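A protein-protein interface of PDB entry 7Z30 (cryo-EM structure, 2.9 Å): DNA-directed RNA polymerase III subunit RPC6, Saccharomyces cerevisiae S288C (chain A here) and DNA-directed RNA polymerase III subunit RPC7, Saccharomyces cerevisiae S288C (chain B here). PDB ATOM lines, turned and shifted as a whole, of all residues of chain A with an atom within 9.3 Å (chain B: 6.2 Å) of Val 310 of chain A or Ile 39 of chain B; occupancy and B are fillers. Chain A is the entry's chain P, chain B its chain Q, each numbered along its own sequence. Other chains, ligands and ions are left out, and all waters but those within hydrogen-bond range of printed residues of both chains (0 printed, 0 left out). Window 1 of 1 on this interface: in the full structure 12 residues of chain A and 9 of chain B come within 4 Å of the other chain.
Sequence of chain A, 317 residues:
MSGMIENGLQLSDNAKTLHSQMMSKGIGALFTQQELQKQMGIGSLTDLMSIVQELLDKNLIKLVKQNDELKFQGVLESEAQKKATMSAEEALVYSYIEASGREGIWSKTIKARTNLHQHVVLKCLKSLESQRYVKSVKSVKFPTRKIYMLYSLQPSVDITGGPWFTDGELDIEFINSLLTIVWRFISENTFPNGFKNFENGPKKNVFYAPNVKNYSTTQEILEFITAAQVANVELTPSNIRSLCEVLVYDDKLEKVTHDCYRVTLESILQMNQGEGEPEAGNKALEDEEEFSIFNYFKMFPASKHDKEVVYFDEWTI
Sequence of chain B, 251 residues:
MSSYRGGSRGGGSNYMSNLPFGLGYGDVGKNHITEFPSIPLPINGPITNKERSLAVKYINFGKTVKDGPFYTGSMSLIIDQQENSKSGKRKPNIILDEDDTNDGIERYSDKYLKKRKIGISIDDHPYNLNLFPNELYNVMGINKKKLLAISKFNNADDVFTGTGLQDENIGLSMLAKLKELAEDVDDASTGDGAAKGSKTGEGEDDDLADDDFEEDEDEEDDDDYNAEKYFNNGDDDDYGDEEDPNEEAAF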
ATOM      1  N   PRO A 301      21.006   7.807  22.404  1.00  0.00           N
ATOM      2  CA  PRO A 301      21.571   6.573  21.836  1.00  0.00           C
ATOM      3  C   PRO A 301      22.142   6.757  20.439  1.00  0.00           C
ATOM      4  O   PRO A 301      22.064   7.846  19.861  1.00  0.00           O
ATOM      5  CB  PRO A 301      20.374   5.612  21.822  1.00  0.00           C
ATOM      6  CG  PRO A 301      19.165   6.481  21.981  1.00  0.00           C
ATOM      7  CD  PRO A 301      19.610   7.621  22.827  1.00  0.00           C
ATOM      8  N   ALA A 302      22.727   5.687  19.892  1.00  0.00           N
ATOM      9  CA  ALA A 302      23.296   5.760  18.550  1.00  0.00           C
ATOM     10  C   ALA A 302      22.230   6.112  17.521  1.00  0.00           C
ATOM     11  O   ALA A 302      22.496   6.866  16.577  1.00  0.00           O
ATOM     12  CB  ALA A 302      23.975   4.437  18.195  1.00  0.00           C
ATOM     13  N   ASP A 306      23.714   1.299  12.496  1.00  0.00           N
ATOM     14  CA  ASP A 306      25.142   1.038  12.420  1.00  0.00           C
ATOM     15  C   ASP A 306      25.521  -0.124  13.335  1.00  0.00           C
ATOM     16  O   ASP A 306      24.686  -0.727  14.015  1.00  0.00           O
ATOM     17  CB  ASP A 306      25.929   2.295  12.784  1.00  0.00           C
ATOM     18  CG  ASP A 306      25.532   2.861  14.136  1.00  0.00           C
ATOM     19  OD1 ASP A 306      24.516   2.405  14.703  1.00  0.00           O
ATOM     20  OD2 ASP A 306      26.236   3.766  14.634  1.00  0.00           O
ATOM     21  N   LYS A 307      26.810  -0.434  13.351  1.00  0.00           N
ATOM     22  CA  LYS A 307      27.371  -1.495  14.170  1.00  0.00           C
ATOM     23  C   LYS A 307      28.134  -0.873  15.334  1.00  0.00           C
ATOM     24  O   LYS A 307      28.080   0.342  15.558  1.00  0.00           O
ATOM     25  CB  LYS A 307      28.264  -2.403  13.323  1.00  0.00           C
ATOM     26  CG  LYS A 307      27.516  -3.488  12.568  1.00  0.00           C
ATOM     27  CD  LYS A 307      27.094  -2.999  11.193  1.00  0.00           C
ATOM     28  CE  LYS A 307      28.303  -2.755  10.304  1.00  0.00           C
ATOM     29  NZ  LYS A 307      27.912  -2.237   8.965  1.00  0.00           N
ATOM     30  N   GLU A 308      28.827  -1.721  16.095  1.00  0.00           N
ATOM     31  CA  GLU A 308      29.645  -1.338  17.241  1.00  0.00           C
ATOM     32  C   GLU A 308      28.814  -0.824  18.409  1.00  0.00           C
ATOM     33  O   GLU A 308      29.373  -0.251  19.354  1.00  0.00           O
ATOM     34  CB  GLU A 308      30.700  -0.288  16.867  1.00  0.00           C
ATOM     35  CG  GLU A 308      31.788  -0.780  15.918  1.00  0.00           C
ATOM     36  CD  GLU A 308      31.336  -0.837  14.471  1.00  0.00           C
ATOM     37  OE1 GLU A 308      30.971   0.221  13.917  1.00  0.00           O
ATOM     38  OE2 GLU A 308      31.359  -1.939  13.884  1.00  0.00           O
ATOM     39  N   VAL A 309      27.494  -1.008  18.374  1.00  0.00           N
ATOM     40  CA  VAL A 309      26.636  -0.538  19.453  1.00  0.00           C
ATOM     41  C   VAL A 309      26.821  -1.434  20.670  1.00  0.00           C
ATOM     42  O   VAL A 309      27.043  -2.646  20.542  1.00  0.00           O
ATOM     43  CB  VAL A 309      25.168  -0.508  18.999  1.00  0.00           C
ATOM     44  CG1 VAL A 309      24.295   0.185  20.038  1.00  0.00           C
ATOM     45  CG2 VAL A 309      25.045   0.175  17.644  1.00  0.00           C
ATOM     46  N   VAL A 310      26.738  -0.841  21.856  1.00  0.00           N
ATOM     47  CA  VAL A 310      26.924  -1.556  23.112  1.00  0.00           C
ATOM     48  C   VAL A 310      25.577  -1.705  23.801  1.00  0.00           C
ATOM     49  O   VAL A 310      24.730  -0.805  23.768  1.00  0.00           O
ATOM     50  CB  VAL A 310      27.936  -0.830  24.021  1.00  0.00           C
ATOM     51  CG1 VAL A 310      28.455  -1.766  25.102  1.00  0.00           C
ATOM     52  CG2 VAL A 310      29.073  -0.264  23.192  1.00  0.00           C
ATOM     53  N   TYR A 311      25.376  -2.860  24.433  1.00  0.00           N
ATOM     54  CA  TYR A 311      24.152  -3.143  25.168  1.00  0.00           C
ATOM     55  C   TYR A 311      24.528  -3.788  26.490  1.00  0.00           C
ATOM     56  O   TYR A 311      25.424  -4.635  26.540  1.00  0.00           O
ATOM     57  CB  TYR A 311      23.197  -4.054  24.376  1.00  0.00           C
ATOM     58  CG  TYR A 311      23.130  -3.779  22.884  1.00  0.00           C
ATOM     59  CD1 TYR A 311      24.187  -4.101  22.041  1.00  0.00           C
ATOM     60  CD2 TYR A 311      22.008  -3.182  22.324  1.00  0.00           C
ATOM     61  CE1 TYR A 311      24.127  -3.844  20.687  1.00  0.00           C
ATOM     62  CE2 TYR A 311      21.939  -2.921  20.968  1.00  0.00           C
ATOM     63  CZ  TYR A 311      23.003  -3.253  20.156  1.00  0.00           C
ATOM     64  OH  TYR A 311      22.943  -2.998  18.806  1.00  0.00           O
ATOM     65  N   PHE A 312      23.848  -3.377  27.561  1.00  0.00           N
ATOM     66  CA  PHE A 312      24.219  -3.834  28.892  1.00  0.00           C
ATOM     67  C   PHE A 312      23.838  -5.292  29.121  1.00  0.00           C
ATOM     68  O   PHE A 312      24.417  -5.940  29.999  1.00  0.00           O
ATOM     69  CB  PHE A 312      23.571  -2.921  29.941  1.00  0.00           C
ATOM     70  CG  PHE A 312      23.824  -3.338  31.364  1.00  0.00           C
ATOM     71  CD1 PHE A 312      24.939  -2.870  32.040  1.00  0.00           C
ATOM     72  CD2 PHE A 312      22.939  -4.162  32.037  1.00  0.00           C
ATOM     73  CE1 PHE A 312      25.178  -3.236  33.347  1.00  0.00           C
ATOM     74  CE2 PHE A 312      23.178  -4.528  33.346  1.00  0.00           C
ATOM     75  CZ  PHE A 312      24.297  -4.064  34.001  1.00  0.00           C
ATOM     76  N   ASP A 313      22.892  -5.823  28.347  1.00  0.00           N
ATOM     77  CA  ASP A 313      22.432  -7.196  28.500  1.00  0.00           C
ATOM     78  C   ASP A 313      22.971  -8.138  27.430  1.00  0.00           C
ATOM     79  O   ASP A 313      22.480  -9.265  27.315  1.00  0.00           O
ATOM     80  CB  ASP A 313      20.901  -7.242  28.499  1.00  0.00           C
ATOM     81  CG  ASP A 313      20.295  -6.453  27.354  1.00  0.00           C
ATOM     82  OD1 ASP A 313      21.057  -5.823  26.594  1.00  0.00           O
ATOM     83  OD2 ASP A 313      19.055  -6.477  27.209  1.00  0.00           O
ATOM     84  N   GLU A 314      23.960  -7.708  26.641  1.00  0.00           N
ATOM     85  CA  GLU A 314      24.531  -8.587  25.623  1.00  0.00           C
ATOM     86  C   GLU A 314      25.283  -9.755  26.249  1.00  0.00           C
ATOM     87  O   GLU A 314      25.431 -10.812  25.624  1.00  0.00           O
ATOM     88  CB  GLU A 314      25.459  -7.797  24.702  1.00  0.00           C
ATOM     89  CG  GLU A 314      25.680  -8.444  23.344  1.00  0.00           C
ATOM     90  CD  GLU A 314      24.743  -7.918  22.278  1.00  0.00           C
ATOM     91  OE1 GLU A 314      23.634  -8.473  22.136  1.00  0.00           O
ATOM     92  OE2 GLU A 314      25.123  -6.964  21.571  1.00  0.00           O
ATOM     93  N   TRP A 315      25.767  -9.586  27.479  1.00  0.00           N
ATOM     94  CA  TRP A 315      26.560 -10.624  28.125  1.00  0.00           C
ATOM     95  C   TRP A 315      25.703 -11.688  28.801  1.00  0.00           C
ATOM     96  O   TRP A 315      26.244 -12.711  29.232  1.00  0.00           O
ATOM     97  CB  TRP A 315      27.511  -9.981  29.137  1.00  0.00           C
ATOM     98  CG  TRP A 315      28.542 -10.909  29.696  1.00  0.00           C
ATOM     99  CD1 TRP A 315      29.521 -11.553  29.004  1.00  0.00           C
ATOM    100  CD2 TRP A 315      28.722 -11.267  31.071  1.00  0.00           C
ATOM    101  NE1 TRP A 315      30.289 -12.307  29.857  1.00  0.00           N
ATOM    102  CE2 TRP A 315      29.819 -12.146  31.133  1.00  0.00           C
ATOM    103  CE3 TRP A 315      28.056 -10.935  32.254  1.00  0.00           C
ATOM    104  CZ2 TRP A 315      30.267 -12.699  32.332  1.00  0.00           C
ATOM    105  CZ3 TRP A 315      28.502 -11.484  33.443  1.00  0.00           C
ATOM    106  CH2 TRP A 315      29.598 -12.354  33.472  1.00  0.00           C
ATOM    107  N   PRO B  37      19.978  -9.615  23.083  1.00  0.00           N
ATOM    108  CA  PRO B  37      19.275  -8.706  23.995  1.00  0.00           C
ATOM    109  C   PRO B  37      19.595  -7.258  23.662  1.00  0.00           C
ATOM    110  O   PRO B  37      20.747  -6.898  23.417  1.00  0.00           O
ATOM    111  CB  PRO B  37      19.806  -9.109  25.376  1.00  0.00           C
ATOM    112  CG  PRO B  37      20.360 -10.493  25.188  1.00  0.00           C
ATOM    113  CD  PRO B  37      20.909 -10.503  23.799  1.00  0.00           C
ATOM    114  N   SER B  38      18.558  -6.424  23.656  1.00  0.00           N
ATOM    115  CA  SER B  38      18.661  -5.050  23.176  1.00  0.00           C
ATOM    116  C   SER B  38      18.361  -4.081  24.308  1.00  0.00           C
ATOM    117  O   SER B  38      17.208  -3.965  24.742  1.00  0.00           O
ATOM    118  CB  SER B  38      17.711  -4.810  22.001  1.00  0.00           C
ATOM    119  OG  SER B  38      16.373  -4.686  22.446  1.00  0.00           O
ATOM    120  N   ILE B  39      19.393  -3.389  24.778  1.00  0.00           N
ATOM    121  CA  ILE B  39      19.244  -2.244  25.673  1.00  0.00           C
ATOM    122  C   ILE B  39      20.200  -1.167  25.176  1.00  0.00           C
ATOM    123  O   ILE B  39      21.417  -1.271  25.392  1.00  0.00           O
ATOM    124  CB  ILE B  39      19.516  -2.619  27.139  1.00  0.00           C
ATOM    125  CG1 ILE B  39      18.354  -3.432  27.708  1.00  0.00           C
ATOM    126  CG2 ILE B  39      19.715  -1.370  27.986  1.00  0.00           C
ATOM    127  CD1 ILE B  39      18.570  -3.894  29.132  1.00  0.00           C
ATOM    128  N   PRO B  40      19.709  -0.140  24.484  1.00  0.00           N
ATOM    129  CA  PRO B  40      20.616   0.872  23.918  1.00  0.00           C
ATOM    130  C   PRO B  40      21.340   1.639  25.013  1.00  0.00           C
ATOM    131  O   PRO B  40      20.738   2.409  25.764  1.00  0.00           O
ATOM    132  CB  PRO B  40      19.677   1.778  23.111  1.00  0.00           C
ATOM    133  CG  PRO B  40      18.411   0.989  22.937  1.00  0.00           C
ATOM    134  CD  PRO B  40      18.302   0.117  24.142  1.00  0.00           C
ATOM    135  N   LEU B  41      22.650   1.422  25.096  1.00  0.00           N
ATOM    136  CA  LEU B  41      23.454   2.098  26.098  1.00  0.00           C
ATOM    137  C   LEU B  41      23.710   3.547  25.682  1.00  0.00           C
ATOM    138  O   LEU B  41      24.016   3.822  24.520  1.00  0.00           O
ATOM    139  CB  LEU B  41      24.778   1.368  26.300  1.00  0.00           C
ATOM    140  CG  LEU B  41      25.339   1.331  27.723  1.00  0.00           C
ATOM    141  CD1 LEU B  41      24.320   0.746  28.685  1.00  0.00           C
ATOM    142  CD2 LEU B  41      26.633   0.536  27.765  1.00  0.00           C
ATOM    143  N   PRO B  42      23.597   4.490  26.616  1.00  0.00           N
ATOM    144  CA  PRO B  42      23.787   5.910  26.288  1.00  0.00           C
ATOM    145  C   PRO B  42      25.237   6.357  26.169  1.00  0.00           C
ATOM    146  O   PRO B  42      25.487   7.566  26.168  1.00  0.00           O
ATOM    147  CB  PRO B  42      23.111   6.608  27.475  1.00  0.00           C
ATOM    148  CG  PRO B  42      23.337   5.682  28.615  1.00  0.00           C
ATOM    149  CD  PRO B  42      23.299   4.285  28.045  1.00  0.00           C
ATOM    150  N   ILE B  43      26.187   5.432  26.069  1.00  0.00           N
ATOM    151  CA  ILE B  43      27.596   5.774  25.934  1.00  0.00           C
ATOM    152  C   ILE B  43      27.968   6.041  24.473  1.00  0.00           C
ATOM    153  O   ILE B  43      29.145   6.198  24.151  1.00  0.00           O
ATOM    154  CB  ILE B  43      28.497   4.699  26.563  1.00  0.00           C
ATOM    155  CG1 ILE B  43      28.536   3.431  25.706  1.00  0.00           C
ATOM    156  CG2 ILE B  43      28.027   4.369  27.971  1.00  0.00           C
ATOM    157  CD1 ILE B  43      29.835   3.230  24.952  1.00  0.00           C
ATOM    158  N   ASN B  44      26.977   6.116  23.587  1.00  0.00           N
ATOM    159  CA  ASN B  44      27.185   6.393  22.170  1.00  0.00           C
ATOM    160  C   ASN B  44      26.645   7.772  21.797  1.00  0.00           C
ATOM    161  O   ASN B  44      25.985   7.944  20.770  1.00  0.00           O
ATOM    162  CB  ASN B  44      26.536   5.314  21.309  1.00  0.00           C
ATOM    163  CG  ASN B  44      25.164   4.922  21.809  1.00  0.00           C
ATOM    164  OD1 ASN B  44      24.520   5.679  22.534  1.00  0.00           O
ATOM    165  ND2 ASN B  44      24.709   3.733  21.429  1.00  0.00           N
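The backbone NH of Ala 302 of chain A lies close to the side-chain amide nitrogen of Asn 44 of chain B (3.2 Å). O of Val 310 of chain A is in hydrogen-bond range of N of Leu 41 of chain B (3.3 Å). The backbone NH of Ile 39 of chain B is in hydrogen-bond range of the side-chain carboxylate of Asp 313 of chain A (3.5 Å). O of Pro 37 of chain B lies close to OD1 of Asp 313 of chain A (3.4 Å).
OD1 of Asn 44 of chain B lies close to O of Leu 41 of chain B (2.8 Å).
Printed residues of chain B within 4 Å of Val 310 of chain A: Ile 39 (3.7 Å), Leu 41 (3.3 Å) and Ile 43 (3.99 Å). Of chain A, only Val 310 (3.7 Å), Tyr 311 (3.3 Å), Phe 312 (3.9 Å) and Asp 313 (3.2 Å) come within 4 Å of Ile 39 of chain B. No residue of chain A comes within 4 Å of Pro 40 of chain B. Of chain A, only Val 310 and Phe 312 come within 4 Å of Leu 41 of chain B. Of the printed residues of chain B, Asp 313 of chain A touches Pro 37, Ser 38 and Ile 39. Of the printed residues of chain B, Phe 312 of chain A touches Ile 39 (3.9 Å) and Leu 41 (3.9 Å). Printed residues of chain B within 4 Å of Ala 302 of chain A: Asn 44. Printed residues of chain A within 4 Å of Ile 43 of chain B: Val 310 (3.99 Å). Printed residues of chain B within 4 Å of Pro 301 of chain A: Asn 44 (3.2 Å). Asp 306 of chain A touches none of the printed residues of chain B. The nearest printed residue of chain B that does not touch Val 310 of chain A is Pro 40 of chain B (4.4 Å). The nearest printed residue of chain A that does not touch Ile 43 of chain B is Pro 301 of chain A (6.4 Å).
Hydrophobic or aromatic side chains of chain A that line the printed part of chain B: Ala 302, Val 309, Val 310, Tyr 311 and Phe 312. Of the 8 printed residues of chain B, 6 touch a printed residue of chain A. Among the printed residues, 15 pairs touch across the chains. Among the printed residues, no Asp or Glu carboxylate lies within 4 Å of a Lys or Arg side-chain nitrogen of the other chain.
Among the printed residues, pairs that only touch across the chains: Pro 301 of chain A with Asn 44 of chain B, Val 309 of chain A with Asn 44 of chain B, Val 310 of chain A with Ile 39 of chain B, Val 310 of chain A with Ile 43 of chain B, Tyr 311 of chain A with Pro 37 of chain B, Tyr 311 of chain A with Ser 38 of chain B, Tyr 311 of chain A with Ile 39 of chain B, Phe 312 of chain A with Ile 39 of chain B, Phe 312 of chain A with Leu 41 of chain B, Asp 313 of chain A with Ser 38 of chain B and Glu 314 of chain A with Pro 37 of chain B.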
